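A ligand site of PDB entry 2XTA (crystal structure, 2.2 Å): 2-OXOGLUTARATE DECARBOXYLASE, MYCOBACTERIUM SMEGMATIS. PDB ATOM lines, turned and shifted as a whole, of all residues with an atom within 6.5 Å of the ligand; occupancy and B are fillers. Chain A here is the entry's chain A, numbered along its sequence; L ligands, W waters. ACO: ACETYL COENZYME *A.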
ATOM      1  N   LEU A 472      10.620 -33.147  29.130  1.00  0.00           N
ATOM      2  CA  LEU A 472      11.797 -32.275  29.103  1.00  0.00           C
ATOM      3  C   LEU A 472      11.463 -30.839  29.572  1.00  0.00           C
ATOM      4  O   LEU A 472      10.327 -30.384  29.402  1.00  0.00           O
ATOM      5  CB  LEU A 472      12.424 -32.230  27.708  1.00  0.00           C
ATOM      6  N   MET A 678      -0.304 -33.958  14.043  1.00  0.00           N
ATOM      7  CA  MET A 678       0.363 -32.638  14.117  1.00  0.00           C
ATOM      8  C   MET A 678       0.058 -31.902  15.407  1.00  0.00           C
ATOM      9  O   MET A 678      -0.906 -32.232  16.101  1.00  0.00           O
ATOM     10  CB  MET A 678      -0.119 -31.727  12.979  1.00  0.00           C
ATOM     11  CG  MET A 678       0.006 -32.312  11.574  1.00  0.00           C
ATOM     12  SD  MET A 678      -0.513 -31.154  10.307  1.00  0.00           S
ATOM     13  CE  MET A 678      -2.305 -31.139  10.517  1.00  0.00           C
ATOM     14  N   THR A 679       0.838 -30.836  15.699  1.00  0.00           N
ATOM     15  CA  THR A 679       0.525 -29.921  16.813  1.00  0.00           C
ATOM     16  C   THR A 679       0.047 -28.650  16.156  1.00  0.00           C
ATOM     17  O   THR A 679       0.678 -28.203  15.194  1.00  0.00           O
ATOM     18  CB  THR A 679       1.705 -29.726  17.788  1.00  0.00           C
ATOM     19  OG1 THR A 679       2.118 -31.010  18.262  1.00  0.00           O
ATOM     20  CG2 THR A 679       1.335 -28.842  18.993  1.00  0.00           C
ATOM     21  N   ILE A 680      -1.095 -28.102  16.596  1.00  0.00           N
ATOM     22  CA  ILE A 680      -1.653 -26.870  16.037  1.00  0.00           C
ATOM     23  C   ILE A 680      -1.785 -25.879  17.183  1.00  0.00           C
ATOM     24  O   ILE A 680      -2.495 -26.172  18.159  1.00  0.00           O
ATOM     25  CB  ILE A 680      -2.978 -27.091  15.256  1.00  0.00           C
ATOM     26  CG1 ILE A 680      -2.782 -28.105  14.062  1.00  0.00           C
ATOM     27  CG2 ILE A 680      -3.584 -25.755  14.779  1.00  0.00           C
ATOM     28  CD1 ILE A 680      -4.073 -28.666  13.471  1.00  0.00           C
ATOM     29  N   ARG A 695       9.952 -26.732  23.218  1.00  0.00           N
ATOM     30  CA  ARG A 695       9.379 -28.065  23.449  1.00  0.00           C
ATOM     31  C   ARG A 695       9.449 -28.850  22.132  1.00  0.00           C
ATOM     32  O   ARG A 695       9.955 -29.958  22.122  1.00  0.00           O
ATOM     33  CB  ARG A 695       7.923 -27.991  23.989  1.00  0.00           C
ATOM     34  CG  ARG A 695       7.286 -29.373  24.303  1.00  0.00           C
ATOM     35  CD  ARG A 695       5.823 -29.271  24.756  1.00  0.00           C
ATOM     36  NE  ARG A 695       4.932 -28.831  23.670  1.00  0.00           N
ATOM     37  CZ  ARG A 695       3.602 -28.751  23.756  1.00  0.00           C
ATOM     38  NH1 ARG A 695       2.979 -29.057  24.884  1.00  0.00           N
ATOM     39  NH2 ARG A 695       2.894 -28.332  22.717  1.00  0.00           N
ATOM     40  N   ASP A 699      11.522 -32.213  22.418  1.00  0.00           N
ATOM     41  CA  ASP A 699      10.643 -33.331  22.800  1.00  0.00           C
ATOM     42  C   ASP A 699      10.929 -34.679  22.083  1.00  0.00           C
ATOM     43  O   ASP A 699      10.403 -35.707  22.495  1.00  0.00           O
ATOM     44  CB  ASP A 699       9.149 -32.957  22.637  1.00  0.00           C
ATOM     45  CG  ASP A 699       8.661 -32.623  21.234  1.00  0.00           C
ATOM     46  OD1 ASP A 699       9.401 -32.928  20.257  1.00  0.00           O
ATOM     47  OD2 ASP A 699       7.549 -32.058  21.110  1.00  0.00           O
ATOM     48  N   ILE A 701       9.599 -35.786  19.454  1.00  0.00           N
ATOM     49  CA  ILE A 701       8.369 -36.196  18.755  1.00  0.00           C
ATOM     50  C   ILE A 701       8.477 -35.641  17.323  1.00  0.00           C
ATOM     51  O   ILE A 701       8.362 -34.420  17.147  1.00  0.00           O
ATOM     52  CB  ILE A 701       7.089 -35.699  19.500  1.00  0.00           C
ATOM     53  CG1 ILE A 701       6.972 -36.351  20.904  1.00  0.00           C
ATOM     54  CG2 ILE A 701       5.816 -35.953  18.678  1.00  0.00           C
ATOM     55  CD1 ILE A 701       6.131 -35.576  21.890  1.00  0.00           C
ATOM     56  N   LYS A 730       7.004 -23.102  31.719  1.00  0.00           N
ATOM     57  CA  LYS A 730       7.001 -24.024  30.590  1.00  0.00           C
ATOM     58  C   LYS A 730       5.807 -23.684  29.700  1.00  0.00           C
ATOM     59  O   LYS A 730       5.034 -22.790  30.037  1.00  0.00           O
ATOM     60  CB  LYS A 730       6.983 -25.494  31.077  1.00  0.00           C
ATOM     61  CG  LYS A 730       5.745 -25.858  31.920  1.00  0.00           C
ATOM     62  CD  LYS A 730       5.657 -27.354  32.175  1.00  0.00           C
ATOM     63  CE  LYS A 730       4.381 -27.717  32.887  1.00  0.00           C
ATOM     64  NZ  LYS A 730       3.305 -28.131  31.950  1.00  0.00           N
ATOM     65  N   PHE A 731       5.621 -24.415  28.603  1.00  0.00           N
ATOM     66  CA  PHE A 731       4.499 -24.185  27.706  1.00  0.00           C
ATOM     67  C   PHE A 731       3.189 -24.453  28.432  1.00  0.00           C
ATOM     68  O   PHE A 731       3.033 -25.470  29.101  1.00  0.00           O
ATOM     69  CB  PHE A 731       4.608 -25.051  26.414  1.00  0.00           C
ATOM     70  CG  PHE A 731       3.431 -24.826  25.489  1.00  0.00           C
ATOM     71  CD1 PHE A 731       3.295 -23.627  24.796  1.00  0.00           C
ATOM     72  CD2 PHE A 731       2.416 -25.765  25.393  1.00  0.00           C
ATOM     73  CE1 PHE A 731       2.172 -23.380  23.992  1.00  0.00           C
ATOM     74  CE2 PHE A 731       1.291 -25.522  24.598  1.00  0.00           C
ATOM     75  CZ  PHE A 731       1.185 -24.331  23.903  1.00  0.00           C
ATOM     76  N   ARG A 732       2.251 -23.512  28.278  1.00  0.00           N
ATOM     77  CA  ARG A 732       0.928 -23.591  28.863  1.00  0.00           C
ATOM     78  C   ARG A 732      -0.068 -23.707  27.728  1.00  0.00           C
ATOM     79  O   ARG A 732      -0.178 -22.788  26.902  1.00  0.00           O
ATOM     80  CB  ARG A 732       0.627 -22.359  29.759  1.00  0.00           C
ATOM     81  CG  ARG A 732       1.690 -22.043  30.829  1.00  0.00           C
ATOM     82  CD  ARG A 732       1.634 -22.949  32.038  1.00  0.00           C
ATOM     83  NE  ARG A 732       2.558 -22.504  33.095  1.00  0.00           N
ATOM     84  CZ  ARG A 732       2.881 -23.204  34.176  1.00  0.00           C
ATOM     85  NH1 ARG A 732       2.363 -24.415  34.374  1.00  0.00           N
ATOM     86  NH2 ARG A 732       3.728 -22.708  35.065  1.00  0.00           N
ATOM     87  N   SER A 733      -0.749 -24.860  27.645  1.00  0.00           N
ATOM     88  CA  SER A 733      -1.739 -25.144  26.605  1.00  0.00           C
ATOM     89  C   SER A 733      -3.050 -24.397  26.864  1.00  0.00           C
ATOM     90  O   SER A 733      -3.789 -24.134  25.922  1.00  0.00           O
ATOM     91  CB  SER A 733      -1.992 -26.647  26.520  1.00  0.00           C
ATOM     92  OG  SER A 733      -2.418 -27.185  27.753  1.00  0.00           O
ATOM     93  N   VAL A 734      -3.333 -24.072  28.120  1.00  0.00           N
ATOM     94  CA  VAL A 734      -4.521 -23.324  28.552  1.00  0.00           C
ATOM     95  C   VAL A 734      -4.020 -22.169  29.454  1.00  0.00           C
ATOM     96  O   VAL A 734      -3.227 -22.419  30.351  1.00  0.00           O
ATOM     97  CB  VAL A 734      -5.570 -24.225  29.268  1.00  0.00           C
ATOM     98  CG1 VAL A 734      -6.767 -23.413  29.768  1.00  0.00           C
ATOM     99  CG2 VAL A 734      -6.045 -25.361  28.354  1.00  0.00           C
ATOM    100  N   GLN A 783      -3.043 -24.309  22.696  1.00  0.00           N
ATOM    101  CA  GLN A 783      -2.849 -25.493  21.876  1.00  0.00           C
ATOM    102  C   GLN A 783      -4.201 -25.955  21.364  1.00  0.00           C
ATOM    103  O   GLN A 783      -4.985 -26.467  22.138  1.00  0.00           O
ATOM    104  CB  GLN A 783      -2.137 -26.600  22.692  1.00  0.00           C
ATOM    105  CG  GLN A 783      -1.777 -27.820  21.859  1.00  0.00           C
ATOM    106  CD  GLN A 783      -1.007 -28.800  22.655  1.00  0.00           C
ATOM    107  OE1 GLN A 783       0.160 -28.576  22.960  1.00  0.00           O
ATOM    108  NE2 GLN A 783      -1.649 -29.897  23.051  1.00  0.00           N
ATOM    109  N   ALA A 785      -4.760 -28.249  18.874  1.00  0.00           N
ATOM    110  CA  ALA A 785      -4.703 -29.654  18.539  1.00  0.00           C
ATOM    111  C   ALA A 785      -3.343 -30.236  18.944  1.00  0.00           C
ATOM    112  O   ALA A 785      -2.330 -29.624  18.616  1.00  0.00           O
ATOM    113  CB  ALA A 785      -4.951 -29.865  17.041  1.00  0.00           C
ATOM    114  N   PRO A 786      -3.278 -31.421  19.605  1.00  0.00           N
ATOM    115  CA  PRO A 786      -4.401 -32.135  20.229  1.00  0.00           C
ATOM    116  C   PRO A 786      -5.026 -31.251  21.329  1.00  0.00           C
ATOM    117  O   PRO A 786      -4.294 -30.510  21.995  1.00  0.00           O
ATOM    118  CB  PRO A 786      -3.741 -33.411  20.790  1.00  0.00           C
ATOM    119  CG  PRO A 786      -2.313 -33.008  21.067  1.00  0.00           C
ATOM    120  CD  PRO A 786      -1.976 -31.957  20.024  1.00  0.00           C
ATOM    121  N   LEU A 787      -6.351 -31.270  21.484  1.00  0.00           N
ATOM    122  CA  LEU A 787      -7.012 -30.458  22.488  1.00  0.00           C
ATOM    123  C   LEU A 787      -6.527 -30.841  23.903  1.00  0.00           C
ATOM    124  O   LEU A 787      -6.461 -32.037  24.215  1.00  0.00           O
ATOM    125  CB  LEU A 787      -8.555 -30.536  22.387  1.00  0.00           C
ATOM    126  CG  LEU A 787      -9.256 -29.371  21.639  1.00  0.00           C
ATOM    127  CD1 LEU A 787     -10.706 -29.707  21.354  1.00  0.00           C
ATOM    128  CD2 LEU A 787      -9.231 -28.080  22.442  1.00  0.00           C
ATOM    129  N   PRO A 788      -6.092 -29.860  24.731  1.00  0.00           N
ATOM    130  CA  PRO A 788      -5.638 -30.201  26.096  1.00  0.00           C
ATOM    131  C   PRO A 788      -6.838 -30.445  27.002  1.00  0.00           C
ATOM    132  O   PRO A 788      -7.188 -29.572  27.793  1.00  0.00           O
ATOM    133  CB  PRO A 788      -4.816 -28.978  26.520  1.00  0.00           C
ATOM    134  CG  PRO A 788      -5.271 -27.837  25.617  1.00  0.00           C
ATOM    135  CD  PRO A 788      -6.104 -28.392  24.511  1.00  0.00           C
ATOM    136  N   ARG A 789      -7.479 -31.629  26.856  1.00  0.00           N
ATOM    137  CA  ARG A 789      -8.712 -32.054  27.524  1.00  0.00           C
ATOM    138  C   ARG A 789      -8.622 -31.924  29.063  1.00  0.00           C
ATOM    139  O   ARG A 789      -9.486 -31.272  29.664  1.00  0.00           O
ATOM    140  CB  ARG A 789      -9.036 -33.498  27.112  1.00  0.00           C
ATOM    141  CG  ARG A 789     -10.385 -34.042  27.616  1.00  0.00           C
ATOM    142  CD  ARG A 789     -10.554 -35.493  27.213  1.00  0.00           C
ATOM    143  NE  ARG A 789     -11.817 -36.087  27.659  1.00  0.00           N
ATOM    144  CZ  ARG A 789     -11.975 -36.797  28.777  1.00  0.00           C
ATOM    145  NH1 ARG A 789     -10.953 -36.969  29.615  1.00  0.00           N
ATOM    146  NH2 ARG A 789     -13.157 -37.309  29.079  1.00  0.00           N
ATOM    147  N   ARG A 790      -7.602 -32.524  29.685  1.00  0.00           N
ATOM    148  CA  ARG A 790      -7.398 -32.524  31.126  1.00  0.00           C
ATOM    149  C   ARG A 790      -7.163 -31.073  31.610  1.00  0.00           C
ATOM    150  O   ARG A 790      -7.896 -30.586  32.477  1.00  0.00           O
ATOM    151  CB  ARG A 790      -6.226 -33.449  31.465  1.00  0.00           C
ATOM    152  CG  ARG A 790      -5.988 -33.723  32.939  1.00  0.00           C
ATOM    153  CD  ARG A 790      -4.528 -33.540  33.282  1.00  0.00           C
ATOM    154  NE  ARG A 790      -4.182 -32.116  33.406  1.00  0.00           N
ATOM    155  CZ  ARG A 790      -2.953 -31.630  33.367  1.00  0.00           C
ATOM    156  NH1 ARG A 790      -2.746 -30.320  33.489  1.00  0.00           N
ATOM    157  NH2 ARG A 790      -1.904 -32.435  33.227  1.00  0.00           N
ATOM    158  N   ARG A 791      -6.168 -30.377  31.044  1.00  0.00           N
ATOM    159  CA  ARG A 791      -5.847 -29.006  31.415  1.00  0.00           C
ATOM    160  C   ARG A 791      -7.085 -28.089  31.274  1.00  0.00           C
ATOM    161  O   ARG A 791      -7.298 -27.259  32.144  1.00  0.00           O
ATOM    162  CB  ARG A 791      -4.669 -28.461  30.587  1.00  0.00           C
ATOM    163  CG  ARG A 791      -3.662 -27.778  31.476  1.00  0.00           C
ATOM    164  CD  ARG A 791      -3.136 -26.455  30.956  1.00  0.00           C
ATOM    165  NE  ARG A 791      -1.969 -26.028  31.743  1.00  0.00           N
ATOM    166  CZ  ARG A 791      -0.703 -26.242  31.382  1.00  0.00           C
ATOM    167  NH1 ARG A 791       0.283 -25.864  32.179  1.00  0.00           N
ATOM    168  NH2 ARG A 791      -0.422 -26.834  30.223  1.00  0.00           N
ATOM    169  N   LEU A 792      -7.916 -28.294  30.223  1.00  0.00           N
ATOM    170  CA  LEU A 792      -9.140 -27.531  30.009  1.00  0.00           C
ATOM    171  C   LEU A 792     -10.137 -27.797  31.136  1.00  0.00           C
ATOM    172  O   LEU A 792     -10.647 -26.829  31.717  1.00  0.00           O
ATOM    173  CB  LEU A 792      -9.747 -27.845  28.649  1.00  0.00           C
ATOM    174  CG  LEU A 792     -10.702 -26.846  27.999  1.00  0.00           C
ATOM    175  CD1 LEU A 792     -10.264 -25.373  28.203  1.00  0.00           C
ATOM    176  CD2 LEU A 792     -10.815 -27.130  26.493  1.00  0.00           C
HETATM  177  N1A ACO L   1       3.510 -32.203  21.881  1.00  0.00           N
HETATM  178  C2A ACO L   1       4.428 -32.529  22.811  1.00  0.00           C
HETATM  179  N3A ACO L   1       4.085 -32.557  24.115  1.00  0.00           N
HETATM  180  C4A ACO L   1       2.810 -32.308  24.533  1.00  0.00           C
HETATM  181  C5A ACO L   1       1.815 -31.994  23.582  1.00  0.00           C
HETATM  182  C6A ACO L   1       2.211 -31.954  22.211  1.00  0.00           C
HETATM  183  N6A ACO L   1       1.279 -31.636  21.256  1.00  0.00           N
HETATM  184  N7A ACO L   1       0.645 -31.784  24.252  1.00  0.00           N
HETATM  185  C8A ACO L   1       0.837 -31.971  25.530  1.00  0.00           C
HETATM  186  N9A ACO L   1       2.162 -32.291  25.746  1.00  0.00           N
HETATM  187  C1B ACO L   1       2.796 -32.542  27.031  1.00  0.00           C
HETATM  188  C2B ACO L   1       2.816 -31.142  27.717  1.00  0.00           C
HETATM  189  O2B ACO L   1       3.905 -30.297  27.315  1.00  0.00           O
HETATM  190  C3B ACO L   1       2.794 -31.525  29.214  1.00  0.00           C
HETATM  191  O3B ACO L   1       4.111 -31.908  29.664  1.00  0.00           O
HETATM  192  P3B ACO L   1       4.215 -31.746  31.304  1.00  0.00           P
HETATM  193  O7A ACO L   1       5.453 -30.723  31.623  1.00  0.00           O
HETATM  194  O8A ACO L   1       2.933 -31.039  31.982  1.00  0.00           O
HETATM  195  O9A ACO L   1       4.376 -33.088  31.887  1.00  0.00           O
HETATM  196  C4B ACO L   1       1.893 -32.795  29.198  1.00  0.00           C
HETATM  197  O4B ACO L   1       1.958 -33.387  27.883  1.00  0.00           O
HETATM  198  C5B ACO L   1       0.463 -32.435  29.606  1.00  0.00           C
HETATM  199  O5B ACO L   1      -0.118 -31.628  28.571  1.00  0.00           O
HETATM  200  P1A ACO L   1      -1.083 -30.424  29.094  1.00  0.00           P
HETATM  201  O1A ACO L   1      -0.819 -30.030  30.656  1.00  0.00           O
HETATM  202  O2A ACO L   1      -0.776 -29.256  28.226  1.00  0.00           O
HETATM  203  O3A ACO L   1      -2.672 -30.703  28.834  1.00  0.00           O
HETATM  204  P2A ACO L   1      -3.321 -32.210  29.000  1.00  0.00           P
HETATM  205  O4A ACO L   1      -4.879 -31.831  29.006  1.00  0.00           O
HETATM  206  O5A ACO L   1      -2.844 -32.943  30.230  1.00  0.00           O
HETATM  207  O6A ACO L   1      -3.001 -33.129  27.625  1.00  0.00           O
HETATM  208  CBP ACO L   1      -3.533 -34.877  26.039  1.00  0.00           C
HETATM  209  CCP ACO L   1      -3.913 -34.226  27.397  1.00  0.00           C
HETATM  210  O   HOH W   1       4.141 -28.098  29.311  1.00  0.00           O
HETATM  211  O   HOH W   2       0.413 -28.882  26.065  1.00  0.00           O
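The guanidinium group (NH1) of Arg 695 lies within hydrogen-bond range of an oxygen (O2B) of the ligand, 2.9 Å away.
N7A of the ligand is in hydrogen-bond range of NE2 of Gln 783.
The guanidinium group of Arg 790 is in salt-bridge range of an oxygen (O5A) of the ligand.
The side-chain hydroxyl of Thr 679 lies within hydrogen-bond range of a nitrogen (N6A) of the ligand, 3.2 Å away.
The side-chain amino group of Lys 730 lies within salt-bridge range of an oxygen (O8A) of the ligand.
N of Arg 791 sits at hydrogen-bond distance from O4A of the ligand, 2.8 Å away.
The side-chain hydroxyl (OG) of Ser 733 lies within hydrogen-bond range of an oxygen (O2A) of the ligand, at 2.7 Å.
N of Arg 789 is in hydrogen-bond range of O4A of the ligand, 3.4 Å away.
NH2 of Arg 791 is in salt-bridge range of O2A of the ligand (3.2 Å).
N of Arg 790 sits at hydrogen-bond distance from O4A of the ligand (2.9 Å).
The guanidinium group (NH2) of Arg 695 sits at hydrogen-bond distance from the side-chain amide oxygen (OE1) of Gln 783, 2.8 Å away.
NH2 of Arg 791 is in hydrogen-bond range of OG of Ser 733 (3.2 Å).
The backbone carbonyl oxygen (O) of Ser 733 sits at hydrogen-bond distance from the backbone NH (N) of Gln 783.
The side-chain amide nitrogen (NE2) of Gln 783 sits at hydrogen-bond distance from the backbone carbonyl oxygen (O) of Pro 786 (2.9 Å).
O4A of the ligand lies close to O of Pro 788, at 3.5 Å.
Asp 699 touches the ligand (OD2 to C2A, 3.6 Å).
CD1 of Ile 701 touches C2A of the ligand (3.6 Å).
Pro 786 touches the ligand.
Of the 21 residues printed, 12 come within 4 Å of the ligand.
The nearest printed residue that does not touch the ligand is Leu 787 (4.5 Å).
Water W2 lies within hydrogen-bond range of an oxygen (O2A) of the ligand (2.5 Å), the guanidinium group of Arg 695 (2.8 Å) and the side-chain amide oxygen of Gln 783 (3.1 Å).
Water W1 lies within hydrogen-bond range of the side-chain amino group of Lys 730 (2.8 Å), the backbone carbonyl oxygen of Phe 731 (2.9 Å) and an oxygen (O2B) of the ligand (3.0 Å).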
